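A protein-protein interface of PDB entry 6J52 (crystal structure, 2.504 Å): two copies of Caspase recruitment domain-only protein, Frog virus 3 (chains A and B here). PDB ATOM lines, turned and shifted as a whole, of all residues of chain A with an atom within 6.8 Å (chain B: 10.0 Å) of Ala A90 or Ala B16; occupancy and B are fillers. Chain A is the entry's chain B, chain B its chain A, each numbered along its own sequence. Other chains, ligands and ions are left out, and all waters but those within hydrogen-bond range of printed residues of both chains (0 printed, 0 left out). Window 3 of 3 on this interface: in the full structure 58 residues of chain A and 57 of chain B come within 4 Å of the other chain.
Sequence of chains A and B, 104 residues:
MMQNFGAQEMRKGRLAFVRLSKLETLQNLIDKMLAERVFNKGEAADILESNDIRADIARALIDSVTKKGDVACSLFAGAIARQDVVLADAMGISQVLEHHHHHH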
ATOM      1  N   VAL A  85     -14.914 -14.890  27.292  1.00  0.00           N
ATOM      2  CA  VAL A  85     -15.989 -15.355  26.416  1.00  0.00           C
ATOM      3  C   VAL A  85     -16.930 -14.213  26.025  1.00  0.00           C
ATOM      4  O   VAL A  85     -17.500 -14.227  24.927  1.00  0.00           O
ATOM      5  CB  VAL A  85     -16.747 -16.526  27.081  1.00  0.00           C
ATOM      6  CG1 VAL A  85     -17.680 -16.031  28.199  1.00  0.00           C
ATOM      7  CG2 VAL A  85     -17.518 -17.324  26.035  1.00  0.00           C
ATOM      8  N   VAL A  86     -17.101 -13.210  26.895  1.00  0.00           N
ATOM      9  CA  VAL A  86     -17.966 -12.070  26.583  1.00  0.00           C
ATOM     10  C   VAL A  86     -17.327 -11.186  25.514  1.00  0.00           C
ATOM     11  O   VAL A  86     -17.993 -10.714  24.585  1.00  0.00           O
ATOM     12  CB  VAL A  86     -18.274 -11.259  27.858  1.00  0.00           C
ATOM     13  CG1 VAL A  86     -19.141 -10.041  27.529  1.00  0.00           C
ATOM     14  CG2 VAL A  86     -18.959 -12.120  28.882  1.00  0.00           C
ATOM     15  N   LEU A  87     -16.030 -10.922  25.648  1.00  0.00           N
ATOM     16  CA  LEU A  87     -15.324 -10.205  24.595  1.00  0.00           C
ATOM     17  C   LEU A  87     -15.386 -10.979  23.282  1.00  0.00           C
ATOM     18  O   LEU A  87     -15.656 -10.403  22.216  1.00  0.00           O
ATOM     19  CB  LEU A  87     -13.884  -9.952  25.038  1.00  0.00           C
ATOM     20  CG  LEU A  87     -13.029  -8.928  24.316  1.00  0.00           C
ATOM     21  CD1 LEU A  87     -13.694  -7.554  24.348  1.00  0.00           C
ATOM     22  CD2 LEU A  87     -11.680  -8.892  25.005  1.00  0.00           C
ATOM     23  N   ALA A  88     -15.188 -12.299  23.345  1.00  0.00           N
ATOM     24  CA  ALA A  88     -15.193 -13.094  22.122  1.00  0.00           C
ATOM     25  C   ALA A  88     -16.543 -13.017  21.434  1.00  0.00           C
ATOM     26  O   ALA A  88     -16.614 -12.765  20.227  1.00  0.00           O
ATOM     27  CB  ALA A  88     -14.821 -14.544  22.429  1.00  0.00           C
ATOM     28  N   ASP A  89     -17.631 -13.188  22.204  1.00  0.00           N
ATOM     29  CA  ASP A  89     -18.981 -13.095  21.652  1.00  0.00           C
ATOM     30  C   ASP A  89     -19.260 -11.713  21.078  1.00  0.00           C
ATOM     31  O   ASP A  89     -19.874 -11.582  20.014  1.00  0.00           O
ATOM     32  CB  ASP A  89     -20.017 -13.415  22.726  1.00  0.00           C
ATOM     33  CG  ASP A  89     -21.427 -13.582  22.154  1.00  0.00           C
ATOM     34  OD1 ASP A  89     -22.128 -12.561  21.950  1.00  0.00           O
ATOM     35  OD2 ASP A  89     -21.832 -14.743  21.922  1.00  0.00           O
ATOM     36  N   ALA A  90     -18.835 -10.668  21.780  1.00  0.00           N
ATOM     37  CA  ALA A  90     -19.164  -9.324  21.334  1.00  0.00           C
ATOM     38  C   ALA A  90     -18.465  -8.977  20.023  1.00  0.00           C
ATOM     39  O   ALA A  90     -19.006  -8.203  19.224  1.00  0.00           O
ATOM     40  CB  ALA A  90     -18.821  -8.319  22.433  1.00  0.00           C
ATOM     41  N   MET A  91     -17.281  -9.537  19.777  1.00  0.00           N
ATOM     42  CA  MET A  91     -16.527  -9.248  18.558  1.00  0.00           C
ATOM     43  C   MET A  91     -16.831 -10.205  17.409  1.00  0.00           C
ATOM     44  O   MET A  91     -16.252 -10.046  16.330  1.00  0.00           O
ATOM     45  CB  MET A  91     -15.023  -9.283  18.843  1.00  0.00           C
ATOM     46  CG  MET A  91     -14.555  -8.363  19.961  1.00  0.00           C
ATOM     47  SD  MET A  91     -12.846  -8.727  20.427  1.00  0.00           S
ATOM     48  CE  MET A  91     -12.066  -8.243  18.858  1.00  0.00           C
ATOM     49  N   GLY A  92     -17.705 -11.192  17.599  1.00  0.00           N
ATOM     50  CA  GLY A  92     -17.975 -12.159  16.547  1.00  0.00           C
ATOM     51  C   GLY A  92     -17.078 -13.381  16.529  1.00  0.00           C
ATOM     52  O   GLY A  92     -17.094 -14.136  15.547  1.00  0.00           O
ATOM     53  N   ILE A  93     -16.297 -13.606  17.572  1.00  0.00           N
ATOM     54  CA  ILE A  93     -15.429 -14.775  17.655  1.00  0.00           C
ATOM     55  C   ILE A  93     -16.211 -15.901  18.324  1.00  0.00           C
ATOM     56  O   ILE A  93     -16.898 -15.685  19.331  1.00  0.00           O
ATOM     57  CB  ILE A  93     -14.136 -14.435  18.423  1.00  0.00           C
ATOM     58  CG1 ILE A  93     -13.511 -13.161  17.839  1.00  0.00           C
ATOM     59  CG2 ILE A  93     -13.138 -15.577  18.359  1.00  0.00           C
ATOM     60  CD1 ILE A  93     -12.476 -12.532  18.711  1.00  0.00           C
ATOM     61  N   PHE B   5     -10.529 -15.791  11.433  1.00  0.00           N
ATOM     62  CA  PHE B   5     -11.053 -14.479  11.816  1.00  0.00           C
ATOM     63  C   PHE B   5     -10.030 -13.436  11.356  1.00  0.00           C
ATOM     64  O   PHE B   5      -8.974 -13.307  11.975  1.00  0.00           O
ATOM     65  CB  PHE B   5     -11.271 -14.430  13.334  1.00  0.00           C
ATOM     66  CG  PHE B   5     -11.989 -13.202  13.833  1.00  0.00           C
ATOM     67  CD1 PHE B   5     -13.382 -13.192  13.957  1.00  0.00           C
ATOM     68  CD2 PHE B   5     -11.276 -12.067  14.225  1.00  0.00           C
ATOM     69  CE1 PHE B   5     -14.061 -12.059  14.444  1.00  0.00           C
ATOM     70  CE2 PHE B   5     -11.954 -10.932  14.708  1.00  0.00           C
ATOM     71  CZ  PHE B   5     -13.348 -10.935  14.814  1.00  0.00           C
ATOM     72  N   GLU B   9     -12.778  -8.753   9.788  1.00  0.00           N
ATOM     73  CA  GLU B   9     -13.604  -9.056  10.949  1.00  0.00           C
ATOM     74  C   GLU B   9     -13.084  -8.367  12.210  1.00  0.00           C
ATOM     75  O   GLU B   9     -13.877  -8.044  13.102  1.00  0.00           O
ATOM     76  CB  GLU B   9     -13.693 -10.571  11.148  1.00  0.00           C
ATOM     77  CG  GLU B   9     -14.313 -11.334   9.956  1.00  0.00           C
ATOM     78  CD  GLU B   9     -13.689 -12.721   9.735  1.00  0.00           C
ATOM     79  OE1 GLU B   9     -14.377 -13.742   9.977  1.00  0.00           O
ATOM     80  OE2 GLU B   9     -12.507 -12.788   9.316  1.00  0.00           O
ATOM     81  N   MET B  10     -11.770  -8.129  12.305  1.00  0.00           N
ATOM     82  CA  MET B  10     -11.232  -7.437  13.471  1.00  0.00           C
ATOM     83  C   MET B  10     -11.590  -5.956  13.452  1.00  0.00           C
ATOM     84  O   MET B  10     -11.870  -5.380  14.513  1.00  0.00           O
ATOM     85  CB  MET B  10      -9.715  -7.631  13.565  1.00  0.00           C
ATOM     86  CG  MET B  10      -9.074  -7.219  14.908  1.00  0.00           C
ATOM     87  SD  MET B  10      -9.360  -8.342  16.309  1.00  0.00           S
ATOM     88  CE  MET B  10      -8.836  -9.912  15.611  1.00  0.00           C
ATOM     89  N   ARG B  11     -11.611  -5.326  12.268  1.00  0.00           N
ATOM     90  CA  ARG B  11     -12.113  -3.955  12.185  1.00  0.00           C
ATOM     91  C   ARG B  11     -13.572  -3.861  12.637  1.00  0.00           C
ATOM     92  O   ARG B  11     -13.940  -2.946  13.380  1.00  0.00           O
ATOM     93  CB  ARG B  11     -11.951  -3.402  10.769  1.00  0.00           C
ATOM     94  CG  ARG B  11     -10.517  -3.362  10.281  1.00  0.00           C
ATOM     95  CD  ARG B  11     -10.347  -2.496   9.038  1.00  0.00           C
ATOM     96  NE  ARG B  11      -9.395  -3.104   8.106  1.00  0.00           N
ATOM     97  CZ  ARG B  11      -9.761  -3.910   7.116  1.00  0.00           C
ATOM     98  NH1 ARG B  11     -11.047  -4.197   6.942  1.00  0.00           N
ATOM     99  NH2 ARG B  11      -8.854  -4.435   6.305  1.00  0.00           N
ATOM    100  N   LYS B  12     -14.422  -4.806  12.222  1.00  0.00           N
ATOM    101  CA  LYS B  12     -15.803  -4.765  12.685  1.00  0.00           C
ATOM    102  C   LYS B  12     -15.933  -5.013  14.184  1.00  0.00           C
ATOM    103  O   LYS B  12     -16.943  -4.615  14.771  1.00  0.00           O
ATOM    104  CB  LYS B  12     -16.665  -5.771  11.925  1.00  0.00           C
ATOM    105  CG  LYS B  12     -16.583  -5.638  10.416  1.00  0.00           C
ATOM    106  CD  LYS B  12     -17.041  -6.910   9.700  1.00  0.00           C
ATOM    107  CE  LYS B  12     -17.591  -6.601   8.302  1.00  0.00           C
ATOM    108  NZ  LYS B  12     -17.859  -7.858   7.533  1.00  0.00           N
ATOM    109  N   GLY B  13     -14.949  -5.644  14.821  1.00  0.00           N
ATOM    110  CA  GLY B  13     -15.001  -5.914  16.244  1.00  0.00           C
ATOM    111  C   GLY B  13     -14.254  -4.921  17.112  1.00  0.00           C
ATOM    112  O   GLY B  13     -14.159  -5.130  18.328  1.00  0.00           O
ATOM    113  N   ARG B  14     -13.731  -3.843  16.524  1.00  0.00           N
ATOM    114  CA  ARG B  14     -12.819  -2.947  17.222  1.00  0.00           C
ATOM    115  C   ARG B  14     -13.505  -2.245  18.383  1.00  0.00           C
ATOM    116  O   ARG B  14     -13.006  -2.249  19.509  1.00  0.00           O
ATOM    117  CB  ARG B  14     -12.266  -1.923  16.234  1.00  0.00           C
ATOM    118  CG  ARG B  14     -11.254  -0.972  16.829  1.00  0.00           C
ATOM    119  CD  ARG B  14     -10.667  -0.068  15.747  1.00  0.00           C
ATOM    120  NE  ARG B  14      -9.538   0.705  16.247  1.00  0.00           N
ATOM    121  CZ  ARG B  14      -9.675   1.770  17.025  1.00  0.00           C
ATOM    122  NH1 ARG B  14     -10.902   2.177  17.373  1.00  0.00           N
ATOM    123  NH2 ARG B  14      -8.597   2.421  17.456  1.00  0.00           N
ATOM    124  N   LEU B  15     -14.651  -1.627  18.118  1.00  0.00           N
ATOM    125  CA  LEU B  15     -15.345  -0.877  19.153  1.00  0.00           C
ATOM    126  C   LEU B  15     -15.674  -1.759  20.355  1.00  0.00           C
ATOM    127  O   LEU B  15     -15.490  -1.341  21.503  1.00  0.00           O
ATOM    128  CB  LEU B  15     -16.614  -0.245  18.576  1.00  0.00           C
ATOM    129  CG  LEU B  15     -17.454   0.430  19.660  1.00  0.00           C
ATOM    130  CD1 LEU B  15     -16.631   1.570  20.276  1.00  0.00           C
ATOM    131  CD2 LEU B  15     -18.828   0.910  19.139  1.00  0.00           C
ATOM    132  N   ALA B  16     -16.159  -2.983  20.114  1.00  0.00           N
ATOM    133  CA  ALA B  16     -16.407  -3.902  21.223  1.00  0.00           C
ATOM    134  C   ALA B  16     -15.120  -4.207  21.976  1.00  0.00           C
ATOM    135  O   ALA B  16     -15.112  -4.281  23.209  1.00  0.00           O
ATOM    136  CB  ALA B  16     -17.035  -5.202  20.714  1.00  0.00           C
ATOM    137  N   PHE B  17     -14.018  -4.387  21.253  1.00  0.00           N
ATOM    138  CA  PHE B  17     -12.779  -4.720  21.930  1.00  0.00           C
ATOM    139  C   PHE B  17     -12.298  -3.570  22.812  1.00  0.00           C
ATOM    140  O   PHE B  17     -11.865  -3.789  23.949  1.00  0.00           O
ATOM    141  CB  PHE B  17     -11.722  -5.100  20.905  1.00  0.00           C
ATOM    142  CG  PHE B  17     -10.443  -5.496  21.519  1.00  0.00           C
ATOM    143  CD1 PHE B  17     -10.318  -6.724  22.125  1.00  0.00           C
ATOM    144  CD2 PHE B  17      -9.378  -4.616  21.551  1.00  0.00           C
ATOM    145  CE1 PHE B  17      -9.124  -7.100  22.712  1.00  0.00           C
ATOM    146  CE2 PHE B  17      -8.193  -4.978  22.146  1.00  0.00           C
ATOM    147  CZ  PHE B  17      -8.063  -6.228  22.726  1.00  0.00           C
ATOM    148  N   VAL B  18     -12.378  -2.338  22.309  1.00  0.00           N
ATOM    149  CA  VAL B  18     -11.921  -1.185  23.078  1.00  0.00           C
ATOM    150  C   VAL B  18     -12.815  -0.960  24.295  1.00  0.00           C
ATOM    151  O   VAL B  18     -12.332  -0.658  25.393  1.00  0.00           O
ATOM    152  CB  VAL B  18     -11.861   0.059  22.168  1.00  0.00           C
ATOM    153  CG1 VAL B  18     -11.581   1.329  22.984  1.00  0.00           C
ATOM    154  CG2 VAL B  18     -10.817  -0.142  21.075  1.00  0.00           C
ATOM    155  N   ARG B  19     -14.129  -1.125  24.123  1.00  0.00           N
ATOM    156  CA  ARG B  19     -15.073  -0.907  25.216  1.00  0.00           C
ATOM    157  C   ARG B  19     -14.957  -1.977  26.295  1.00  0.00           C
ATOM    158  O   ARG B  19     -15.011  -1.665  27.486  1.00  0.00           O
ATOM    159  CB  ARG B  19     -16.511  -0.915  24.697  1.00  0.00           C
ATOM    160  CG  ARG B  19     -17.050   0.316  24.005  1.00  0.00           C
ATOM    161  CD  ARG B  19     -18.247  -0.106  23.087  1.00  0.00           C
ATOM    162  NE  ARG B  19     -19.291  -0.917  23.748  1.00  0.00           N
ATOM    163  CZ  ARG B  19     -19.932  -1.955  23.192  1.00  0.00           C
ATOM    164  NH1 ARG B  19     -20.865  -2.611  23.884  1.00  0.00           N
ATOM    165  NH2 ARG B  19     -19.635  -2.359  21.960  1.00  0.00           N
ATOM    166  N   LEU B  20     -14.846  -3.250  25.906  1.00  0.00           N
ATOM    167  CA  LEU B  20     -15.158  -4.332  26.832  1.00  0.00           C
ATOM    168  C   LEU B  20     -13.943  -5.041  27.416  1.00  0.00           C
ATOM    169  O   LEU B  20     -14.091  -5.726  28.432  1.00  0.00           O
ATOM    170  CB  LEU B  20     -16.055  -5.373  26.151  1.00  0.00           C
ATOM    171  CG  LEU B  20     -17.402  -4.884  25.620  1.00  0.00           C
ATOM    172  CD1 LEU B  20     -18.184  -6.020  25.031  1.00  0.00           C
ATOM    173  CD2 LEU B  20     -18.201  -4.243  26.731  1.00  0.00           C
ATOM    174  N   SER B  21     -12.759  -4.914  26.816  1.00  0.00           N
ATOM    175  CA  SER B  21     -11.622  -5.690  27.295  1.00  0.00           C
ATOM    176  C   SER B  21     -11.143  -5.175  28.654  1.00  0.00           C
ATOM    177  O   SER B  21     -11.055  -3.964  28.886  1.00  0.00           O
ATOM    178  CB  SER B  21     -10.477  -5.675  26.270  1.00  0.00           C
ATOM    179  OG  SER B  21     -10.157  -4.369  25.816  1.00  0.00           O
ATOM    180  N   LYS B  22     -10.853  -6.099  29.561  1.00  0.00           N
ATOM    181  CA  LYS B  22     -10.291  -5.716  30.846  1.00  0.00           C
ATOM    182  C   LYS B  22      -8.774  -5.583  30.744  1.00  0.00           C
ATOM    183  O   LYS B  22      -8.131  -6.124  29.836  1.00  0.00           O
ATOM    184  CB  LYS B  22     -10.645  -6.738  31.930  1.00  0.00           C
ATOM    185  CG  LYS B  22     -12.085  -7.214  31.922  1.00  0.00           C
ATOM    186  CD  LYS B  22     -13.046  -6.106  32.299  1.00  0.00           C
ATOM    187  CE  LYS B  22     -14.435  -6.674  32.596  1.00  0.00           C
ATOM    188  NZ  LYS B  22     -15.471  -5.595  32.750  1.00  0.00           N
ATOM    189  N   LEU B  26      -5.740  -7.536  28.587  1.00  0.00           N
ATOM    190  CA  LEU B  26      -4.853  -6.890  27.630  1.00  0.00           C
ATOM    191  C   LEU B  26      -3.407  -7.305  27.861  1.00  0.00           C
ATOM    192  O   LEU B  26      -2.668  -7.587  26.907  1.00  0.00           O
ATOM    193  CB  LEU B  26      -5.005  -5.371  27.717  1.00  0.00           C
ATOM    194  CG  LEU B  26      -6.386  -4.854  27.297  1.00  0.00           C
ATOM    195  CD1 LEU B  26      -6.487  -3.352  27.479  1.00  0.00           C
ATOM    196  CD2 LEU B  26      -6.703  -5.259  25.855  1.00  0.00           C
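OG of Ser B21 is in hydrogen-bond range of O of Phe B17, 2.6 Å away.
The backbone NH of Ile A93 is in hydrogen-bond range of the backbone carbonyl oxygen of Ala A88, 2.8 Å away.
CD1 of Leu A87 touches O of Ala B16, 3.7 Å away.
CA of Phe B17 touches CD1 of Leu A87, at 3.8 Å.
CB of Leu B20 touches CD1 of Leu A87, at 3.7 Å.
Ser B21 touches Leu A87 (CB to CD2, 3.7 Å).
O of Ala A90 touches CB of Ala B16, 3.9 Å away.
Met A91 touches Phe B5.
Met A91 touches Met B10 (CE to SD, 3.7 Å).
Gly B13 touches Met A91 (O to CG, 3.6 Å).
Met A91 touches Phe B17.
Phe B5 touches Ile A93.
Of chain A, only Leu A87 (3.7 Å) and Ala A90 (3.9 Å) come within 4 Å of Ala B16.
No residue of chain B comes within 4 Å of Ala A88.
Of chain B, only Phe B5, Met B10, Gly B13 and Phe B17 come within 4 Å of Met A91.
Of the printed residues of chain A, Ser B21 touches Leu A87 (3.7 Å).
Printed residues of chain A within 4 Å of Met B10: Met A91 (3.7 Å).
Arg B11 touches none of the printed residues of chain A.
The nearest residue of chain B that does not touch Ala A90 is Gly B13 (5.5 Å).
The nearest residue of chain A that does not touch Ala B16 is Met A91 (4.1 Å).
Of the 16 printed residues of chain B, 7 touch a printed residue of chain A.
Printed residues of chain B that touch a printed residue of chain A: Phe B5, Met B10, Gly B13, Ala B16, Phe B17, Leu B20 and Ser B21.
Hydrophobic or aromatic side chains of chain B that line the printed part of chain A: Phe B5, Met B10, Ala B16, Phe B17 and Leu B20.
Hydrophobic or aromatic side chains of chain A within 4 Å of the printed part of chain B: Leu A87, Ala A90, Met A91 and Ile A93.
Among the printed residues, no Asp or Glu carboxylate lies within 4 Å of a Lys or Arg side-chain nitrogen of the other chain.
No position is printed for both chains.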
